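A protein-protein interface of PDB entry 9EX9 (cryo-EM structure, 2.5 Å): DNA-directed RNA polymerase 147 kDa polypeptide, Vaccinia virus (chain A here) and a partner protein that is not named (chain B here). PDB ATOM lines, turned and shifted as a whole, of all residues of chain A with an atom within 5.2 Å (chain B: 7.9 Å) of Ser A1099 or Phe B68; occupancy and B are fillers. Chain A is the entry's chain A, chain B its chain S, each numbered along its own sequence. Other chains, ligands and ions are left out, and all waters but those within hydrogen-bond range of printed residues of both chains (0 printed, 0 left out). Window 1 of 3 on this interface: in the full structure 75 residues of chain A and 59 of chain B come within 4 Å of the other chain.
Lys A1097 touches Asn B58.
Phe B68 touches Ser A1099.
Lys A1100 touches Glu B65.
Lys A1100 touches Thr B66 (N to CG2, 3.7 Å).
Of the 7 printed residues of chain A, 4 touch a printed residue of chain B.
Among the printed residues, 5 pairs touch across the chains.
Among the printed residues, no Asp or Glu carboxylate lies within 4 Å of a Lys or Arg side-chain nitrogen of the other chain.
OD1 of Asn B58 is in hydrogen-bond range of N of Ile A1098 (2.5 Å).
Glu A1002 touches none of the printed residues of chain B.
Of the printed residues of chain B, Lys A1097 touches Asn B58 (3.2 Å).
Of the printed residues of chain B, Ile A1098 touches Asn B58 (2.5 Å).
Ser A1099 touches just one residue of chain B: Phe B68 (3.9 Å).
Printed residues of chain A within 4 Å of Asn B58: Lys A1097 and Ile A1098.
Of chain A, only Ser A1099 comes within 4 Å of Phe B68.
Glu B69 touches none of the printed residues of chain A.
The nearest residue of chain A that does not touch Phe B68 is Phe A997 (4.1 Å).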
ATOM      1  N   PHE A 997      33.011  25.883 -14.545  1.00  0.00           N
ATOM      2  CA  PHE A 997      32.387  27.188 -14.369  1.00  0.00           C
ATOM      3  C   PHE A 997      32.589  27.701 -12.950  1.00  0.00           C
ATOM      4  O   PHE A 997      32.278  27.006 -11.980  1.00  0.00           O
ATOM      5  CB  PHE A 997      30.894  27.115 -14.684  1.00  0.00           C
ATOM      6  CG  PHE A 997      30.187  28.430 -14.560  1.00  0.00           C
ATOM      7  CD1 PHE A 997      30.346  29.408 -15.518  1.00  0.00           C
ATOM      8  CD2 PHE A 997      29.359  28.687 -13.486  1.00  0.00           C
ATOM      9  CE1 PHE A 997      29.700  30.614 -15.404  1.00  0.00           C
ATOM     10  CE2 PHE A 997      28.711  29.894 -13.372  1.00  0.00           C
ATOM     11  CZ  PHE A 997      28.884  30.857 -14.331  1.00  0.00           C
ATOM     12  N   GLU A1002      30.464  32.888  -6.228  1.00  0.00           N
ATOM     13  CA  GLU A1002      30.689  31.593  -5.596  1.00  0.00           C
ATOM     14  C   GLU A1002      31.771  31.644  -4.532  1.00  0.00           C
ATOM     15  O   GLU A1002      31.766  30.806  -3.626  1.00  0.00           O
ATOM     16  CB  GLU A1002      31.076  30.550  -6.640  1.00  0.00           C
ATOM     17  CG  GLU A1002      29.911  29.942  -7.382  1.00  0.00           C
ATOM     18  CD  GLU A1002      30.363  29.003  -8.477  1.00  0.00           C
ATOM     19  OE1 GLU A1002      31.587  28.797  -8.601  1.00  0.00           O
ATOM     20  OE2 GLU A1002      29.503  28.475  -9.210  1.00  0.00           O
ATOM     21  N   LYS A1097      32.376  27.096 -19.078  1.00  0.00           N
ATOM     22  CA  LYS A1097      31.096  26.829 -19.716  1.00  0.00           C
ATOM     23  C   LYS A1097      30.003  26.752 -18.663  1.00  0.00           C
ATOM     24  O   LYS A1097      30.145  26.039 -17.667  1.00  0.00           O
ATOM     25  CB  LYS A1097      31.146  25.520 -20.505  1.00  0.00           C
ATOM     26  CG  LYS A1097      31.597  25.663 -21.943  1.00  0.00           C
ATOM     27  CD  LYS A1097      30.414  25.671 -22.889  1.00  0.00           C
ATOM     28  CE  LYS A1097      30.864  25.606 -24.334  1.00  0.00           C
ATOM     29  NZ  LYS A1097      31.741  26.749 -24.692  1.00  0.00           N
ATOM     30  N   ILE A1098      28.908  27.473 -18.893  1.00  0.00           N
ATOM     31  CA  ILE A1098      27.816  27.498 -17.930  1.00  0.00           C
ATOM     32  C   ILE A1098      27.168  26.123 -17.864  1.00  0.00           C
ATOM     33  O   ILE A1098      26.815  25.532 -18.891  1.00  0.00           O
ATOM     34  CB  ILE A1098      26.792  28.579 -18.304  1.00  0.00           C
ATOM     35  CG1 ILE A1098      27.434  29.963 -18.220  1.00  0.00           C
ATOM     36  CG2 ILE A1098      25.587  28.495 -17.386  1.00  0.00           C
ATOM     37  CD1 ILE A1098      26.598  31.063 -18.810  1.00  0.00           C
ATOM     38  N   SER A1099      27.008  25.609 -16.649  1.00  0.00           N
ATOM     39  CA  SER A1099      26.362  24.326 -16.422  1.00  0.00           C
ATOM     40  C   SER A1099      26.237  24.133 -14.921  1.00  0.00           C
ATOM     41  O   SER A1099      26.946  24.769 -14.139  1.00  0.00           O
ATOM     42  CB  SER A1099      27.145  23.172 -17.049  1.00  0.00           C
ATOM     43  OG  SER A1099      27.207  23.302 -18.457  1.00  0.00           O
ATOM     44  N   LYS A1100      25.331  23.246 -14.530  1.00  0.00           N
ATOM     45  CA  LYS A1100      25.040  23.035 -13.121  1.00  0.00           C
ATOM     46  C   LYS A1100      25.944  21.997 -12.468  1.00  0.00           C
ATOM     47  O   LYS A1100      25.810  21.756 -11.266  1.00  0.00           O
ATOM     48  CB  LYS A1100      23.579  22.621 -12.937  1.00  0.00           C
ATOM     49  CG  LYS A1100      23.146  21.429 -13.767  1.00  0.00           C
ATOM     50  CD  LYS A1100      21.844  20.857 -13.240  1.00  0.00           C
ATOM     51  CE  LYS A1100      21.210  19.903 -14.231  1.00  0.00           C
ATOM     52  NZ  LYS A1100      19.943  19.326 -13.708  1.00  0.00           N
ATOM     53  N   PHE A1101      26.859  21.388 -13.217  1.00  0.00           N
ATOM     54  CA  PHE A1101      27.738  20.356 -12.692  1.00  0.00           C
ATOM     55  C   PHE A1101      29.183  20.832 -12.697  1.00  0.00           C
ATOM     56  O   PHE A1101      29.626  21.493 -13.641  1.00  0.00           O
ATOM     57  CB  PHE A1101      27.631  19.070 -13.511  1.00  0.00           C
ATOM     58  CG  PHE A1101      26.271  18.445 -13.485  1.00  0.00           C
ATOM     59  CD1 PHE A1101      25.806  17.815 -12.346  1.00  0.00           C
ATOM     60  CD2 PHE A1101      25.462  18.473 -14.604  1.00  0.00           C
ATOM     61  CE1 PHE A1101      24.554  17.236 -12.323  1.00  0.00           C
ATOM     62  CE2 PHE A1101      24.214  17.895 -14.586  1.00  0.00           C
ATOM     63  CZ  PHE A1101      23.759  17.276 -13.446  1.00  0.00           C
ATOM     64  N   ASN B  58      30.099  31.407 -23.802  1.00  0.00           N
ATOM     65  CA  ASN B  58      28.805  30.753 -23.694  1.00  0.00           C
ATOM     66  C   ASN B  58      27.804  31.469 -24.587  1.00  0.00           C
ATOM     67  O   ASN B  58      27.969  32.642 -24.929  1.00  0.00           O
ATOM     68  CB  ASN B  58      28.291  30.739 -22.250  1.00  0.00           C
ATOM     69  CG  ASN B  58      29.163  29.921 -21.332  1.00  0.00           C
ATOM     70  OD1 ASN B  58      28.856  28.770 -21.030  1.00  0.00           O
ATOM     71  ND2 ASN B  58      30.264  30.510 -20.883  1.00  0.00           N
ATOM     72  N   GLU B  65      18.845  22.547 -17.306  1.00  0.00           N
ATOM     73  CA  GLU B  65      18.427  23.618 -16.410  1.00  0.00           C
ATOM     74  C   GLU B  65      19.406  23.764 -15.253  1.00  0.00           C
ATOM     75  O   GLU B  65      19.976  22.780 -14.786  1.00  0.00           O
ATOM     76  CB  GLU B  65      17.020  23.350 -15.875  1.00  0.00           C
ATOM     77  CG  GLU B  65      15.955  23.280 -16.956  1.00  0.00           C
ATOM     78  CD  GLU B  65      14.574  23.003 -16.399  1.00  0.00           C
ATOM     79  OE1 GLU B  65      14.475  22.600 -15.221  1.00  0.00           O
ATOM     80  OE2 GLU B  65      13.586  23.190 -17.139  1.00  0.00           O
ATOM     81  N   THR B  66      19.595  24.996 -14.793  1.00  0.00           N
ATOM     82  CA  THR B  66      20.539  25.302 -13.730  1.00  0.00           C
ATOM     83  C   THR B  66      19.832  26.036 -12.601  1.00  0.00           C
ATOM     84  O   THR B  66      18.895  26.807 -12.828  1.00  0.00           O
ATOM     85  CB  THR B  66      21.701  26.152 -14.249  1.00  0.00           C
ATOM     86  OG1 THR B  66      21.203  27.410 -14.719  1.00  0.00           O
ATOM     87  CG2 THR B  66      22.418  25.443 -15.384  1.00  0.00           C
ATOM     88  N   LYS B  67      20.299  25.794 -11.375  1.00  0.00           N
ATOM     89  CA  LYS B  67      19.717  26.371 -10.163  1.00  0.00           C
ATOM     90  C   LYS B  67      20.831  27.088  -9.407  1.00  0.00           C
ATOM     91  O   LYS B  67      21.537  26.474  -8.604  1.00  0.00           O
ATOM     92  CB  LYS B  67      19.062  25.297  -9.303  1.00  0.00           C
ATOM     93  CG  LYS B  67      18.037  24.446 -10.031  1.00  0.00           C
ATOM     94  CD  LYS B  67      16.841  25.267 -10.479  1.00  0.00           C
ATOM     95  CE  LYS B  67      15.812  24.406 -11.196  1.00  0.00           C
ATOM     96  NZ  LYS B  67      14.646  25.206 -11.664  1.00  0.00           N
ATOM     97  N   PHE B  68      20.981  28.382  -9.663  1.00  0.00           N
ATOM     98  CA  PHE B  68      21.967  29.203  -8.980  1.00  0.00           C
ATOM     99  C   PHE B  68      21.286  30.014  -7.877  1.00  0.00           C
ATOM    100  O   PHE B  68      20.068  29.966  -7.696  1.00  0.00           O
ATOM    101  CB  PHE B  68      22.694  30.102  -9.978  1.00  0.00           C
ATOM    102  CG  PHE B  68      23.575  29.353 -10.935  1.00  0.00           C
ATOM    103  CD1 PHE B  68      24.788  28.840 -10.522  1.00  0.00           C
ATOM    104  CD2 PHE B  68      23.195  29.166 -12.249  1.00  0.00           C
ATOM    105  CE1 PHE B  68      25.599  28.151 -11.399  1.00  0.00           C
ATOM    106  CE2 PHE B  68      24.006  28.478 -13.128  1.00  0.00           C
ATOM    107  CZ  PHE B  68      25.207  27.973 -12.702  1.00  0.00           C
ATOM    108  N   GLU B  69      22.086  30.781  -7.143  1.00  0.00           N
ATOM    109  CA  GLU B  69      21.627  31.374  -5.895  1.00  0.00           C
ATOM    110  C   GLU B  69      20.628  32.508  -6.089  1.00  0.00           C
ATOM    111  O   GLU B  69      20.083  32.995  -5.096  1.00  0.00           O
ATOM    112  CB  GLU B  69      22.825  31.870  -5.089  1.00  0.00           C
ATOM    113  CG  GLU B  69      22.514  32.160  -3.634  1.00  0.00           C
ATOM    114  CD  GLU B  69      23.761  32.254  -2.780  1.00  0.00           C
ATOM    115  OE1 GLU B  69      24.872  32.132  -3.335  1.00  0.00           O
ATOM    116  OE2 GLU B  69      23.631  32.445  -1.554  1.00  0.00           O
ATOM    117  N   SER B  70      20.380  32.942  -7.321  1.00  0.00           N
ATOM    118  CA  SER B  70      19.439  33.999  -7.693  1.00  0.00           C
ATOM    119  C   SER B  70      19.998  35.390  -7.441  1.00  0.00           C
ATOM    120  O   SER B  70      19.505  36.346  -8.035  1.00  0.00           O
ATOM    121  CB  SER B  70      18.095  33.890  -6.954  1.00  0.00           C
ATOM    122  OG  SER B  70      17.214  34.907  -7.386  1.00  0.00           O
ATOM    123  N   LYS B  71      21.016  35.537  -6.602  1.00  0.00           N
ATOM    124  CA  LYS B  71      21.772  36.777  -6.506  1.00  0.00           C
ATOM    125  C   LYS B  71      22.970  36.777  -7.432  1.00  0.00           C
ATOM    126  O   LYS B  71      23.423  37.844  -7.854  1.00  0.00           O
ATOM    127  CB  LYS B  71      22.244  36.999  -5.067  1.00  0.00           C
ATOM    128  CG  LYS B  71      23.146  35.897  -4.546  1.00  0.00           C
ATOM    129  CD  LYS B  71      23.351  35.975  -3.049  1.00  0.00           C
ATOM    130  CE  LYS B  71      24.286  37.098  -2.667  1.00  0.00           C
ATOM    131  NZ  LYS B  71      24.641  37.031  -1.224  1.00  0.00           N
ATOM    132  N   ASN B  72      23.489  35.594  -7.742  1.00  0.00           N
ATOM    133  CA  ASN B  72      24.482  35.421  -8.786  1.00  0.00           C
ATOM    134  C   ASN B  72      23.860  35.118 -10.137  1.00  0.00           C
ATOM    135  O   ASN B  72      24.525  35.289 -11.161  1.00  0.00           O
ATOM    136  CB  ASN B  72      25.433  34.287  -8.409  1.00  0.00           C
ATOM    137  CG  ASN B  72      26.054  34.487  -7.056  1.00  0.00           C
ATOM    138  OD1 ASN B  72      26.287  35.612  -6.633  1.00  0.00           O
ATOM    139  ND2 ASN B  72      26.320  33.394  -6.360  1.00  0.00           N
ATOM    140  N   ASN B  73      22.605  34.671 -10.163  1.00  0.00           N
ATOM    141  CA  ASN B  73      21.991  34.288 -11.427  1.00  0.00           C
ATOM    142  C   ASN B  73      21.693  35.499 -12.297  1.00  0.00           C
ATOM    143  O   ASN B  73      21.725  35.398 -13.528  1.00  0.00           O
ATOM    144  CB  ASN B  73      20.716  33.493 -11.168  1.00  0.00           C
ATOM    145  CG  ASN B  73      20.104  32.959 -12.435  1.00  0.00           C
ATOM    146  OD1 ASN B  73      19.190  33.558 -12.995  1.00  0.00           O
ATOM    147  ND2 ASN B  73      20.608  31.827 -12.902  1.00  0.00           N
ATOM    148  N   ILE B  74      21.403  36.647 -11.688  1.00  0.00           N
ATOM    149  CA  ILE B  74      21.125  37.847 -12.470  1.00  0.00           C
ATOM    150  C   ILE B  74      22.320  38.191 -13.349  1.00  0.00           C
ATOM    151  O   ILE B  74      22.188  38.371 -14.565  1.00  0.00           O
ATOM    152  CB  ILE B  74      20.751  39.012 -11.538  1.00  0.00           C
ATOM    153  CG1 ILE B  74      19.358  38.781 -10.958  1.00  0.00           C
ATOM    154  CG2 ILE B  74      20.818  40.331 -12.283  1.00  0.00           C
ATOM    155  CD1 ILE B  74      18.987  39.736  -9.864  1.00  0.00           C
ATOM    156  N   ILE B  76      24.807  36.192 -14.110  1.00  0.00           N
ATOM    157  CA  ILE B  76      25.122  35.067 -14.982  1.00  0.00           C
ATOM    158  C   ILE B  76      24.320  35.159 -16.271  1.00  0.00           C
ATOM    159  O   ILE B  76      24.867  35.045 -17.372  1.00  0.00           O
ATOM    160  CB  ILE B  76      24.867  33.739 -14.253  1.00  0.00           C
ATOM    161  CG1 ILE B  76      25.933  33.514 -13.186  1.00  0.00           C
ATOM    162  CG2 ILE B  76      24.858  32.589 -15.240  1.00  0.00           C
ATOM    163  CD1 ILE B  76      25.598  32.421 -12.211  1.00  0.00           C
ATOM    164  N   GLU B  77      23.012  35.373 -16.154  1.00  0.00           N
ATOM    165  CA  GLU B  77      22.177  35.475 -17.341  1.00  0.00           C
ATOM    166  C   GLU B  77      22.360  36.795 -18.070  1.00  0.00           C
ATOM    167  O   GLU B  77      22.103  36.859 -19.275  1.00  0.00           O
ATOM    168  CB  GLU B  77      20.710  35.272 -16.967  1.00  0.00           C
ATOM    169  CG  GLU B  77      20.355  33.807 -16.776  1.00  0.00           C
ATOM    170  CD  GLU B  77      19.119  33.598 -15.932  1.00  0.00           C
ATOM    171  OE1 GLU B  77      18.608  34.585 -15.365  1.00  0.00           O
ATOM    172  OE2 GLU B  77      18.658  32.443 -15.830  1.00  0.00           O
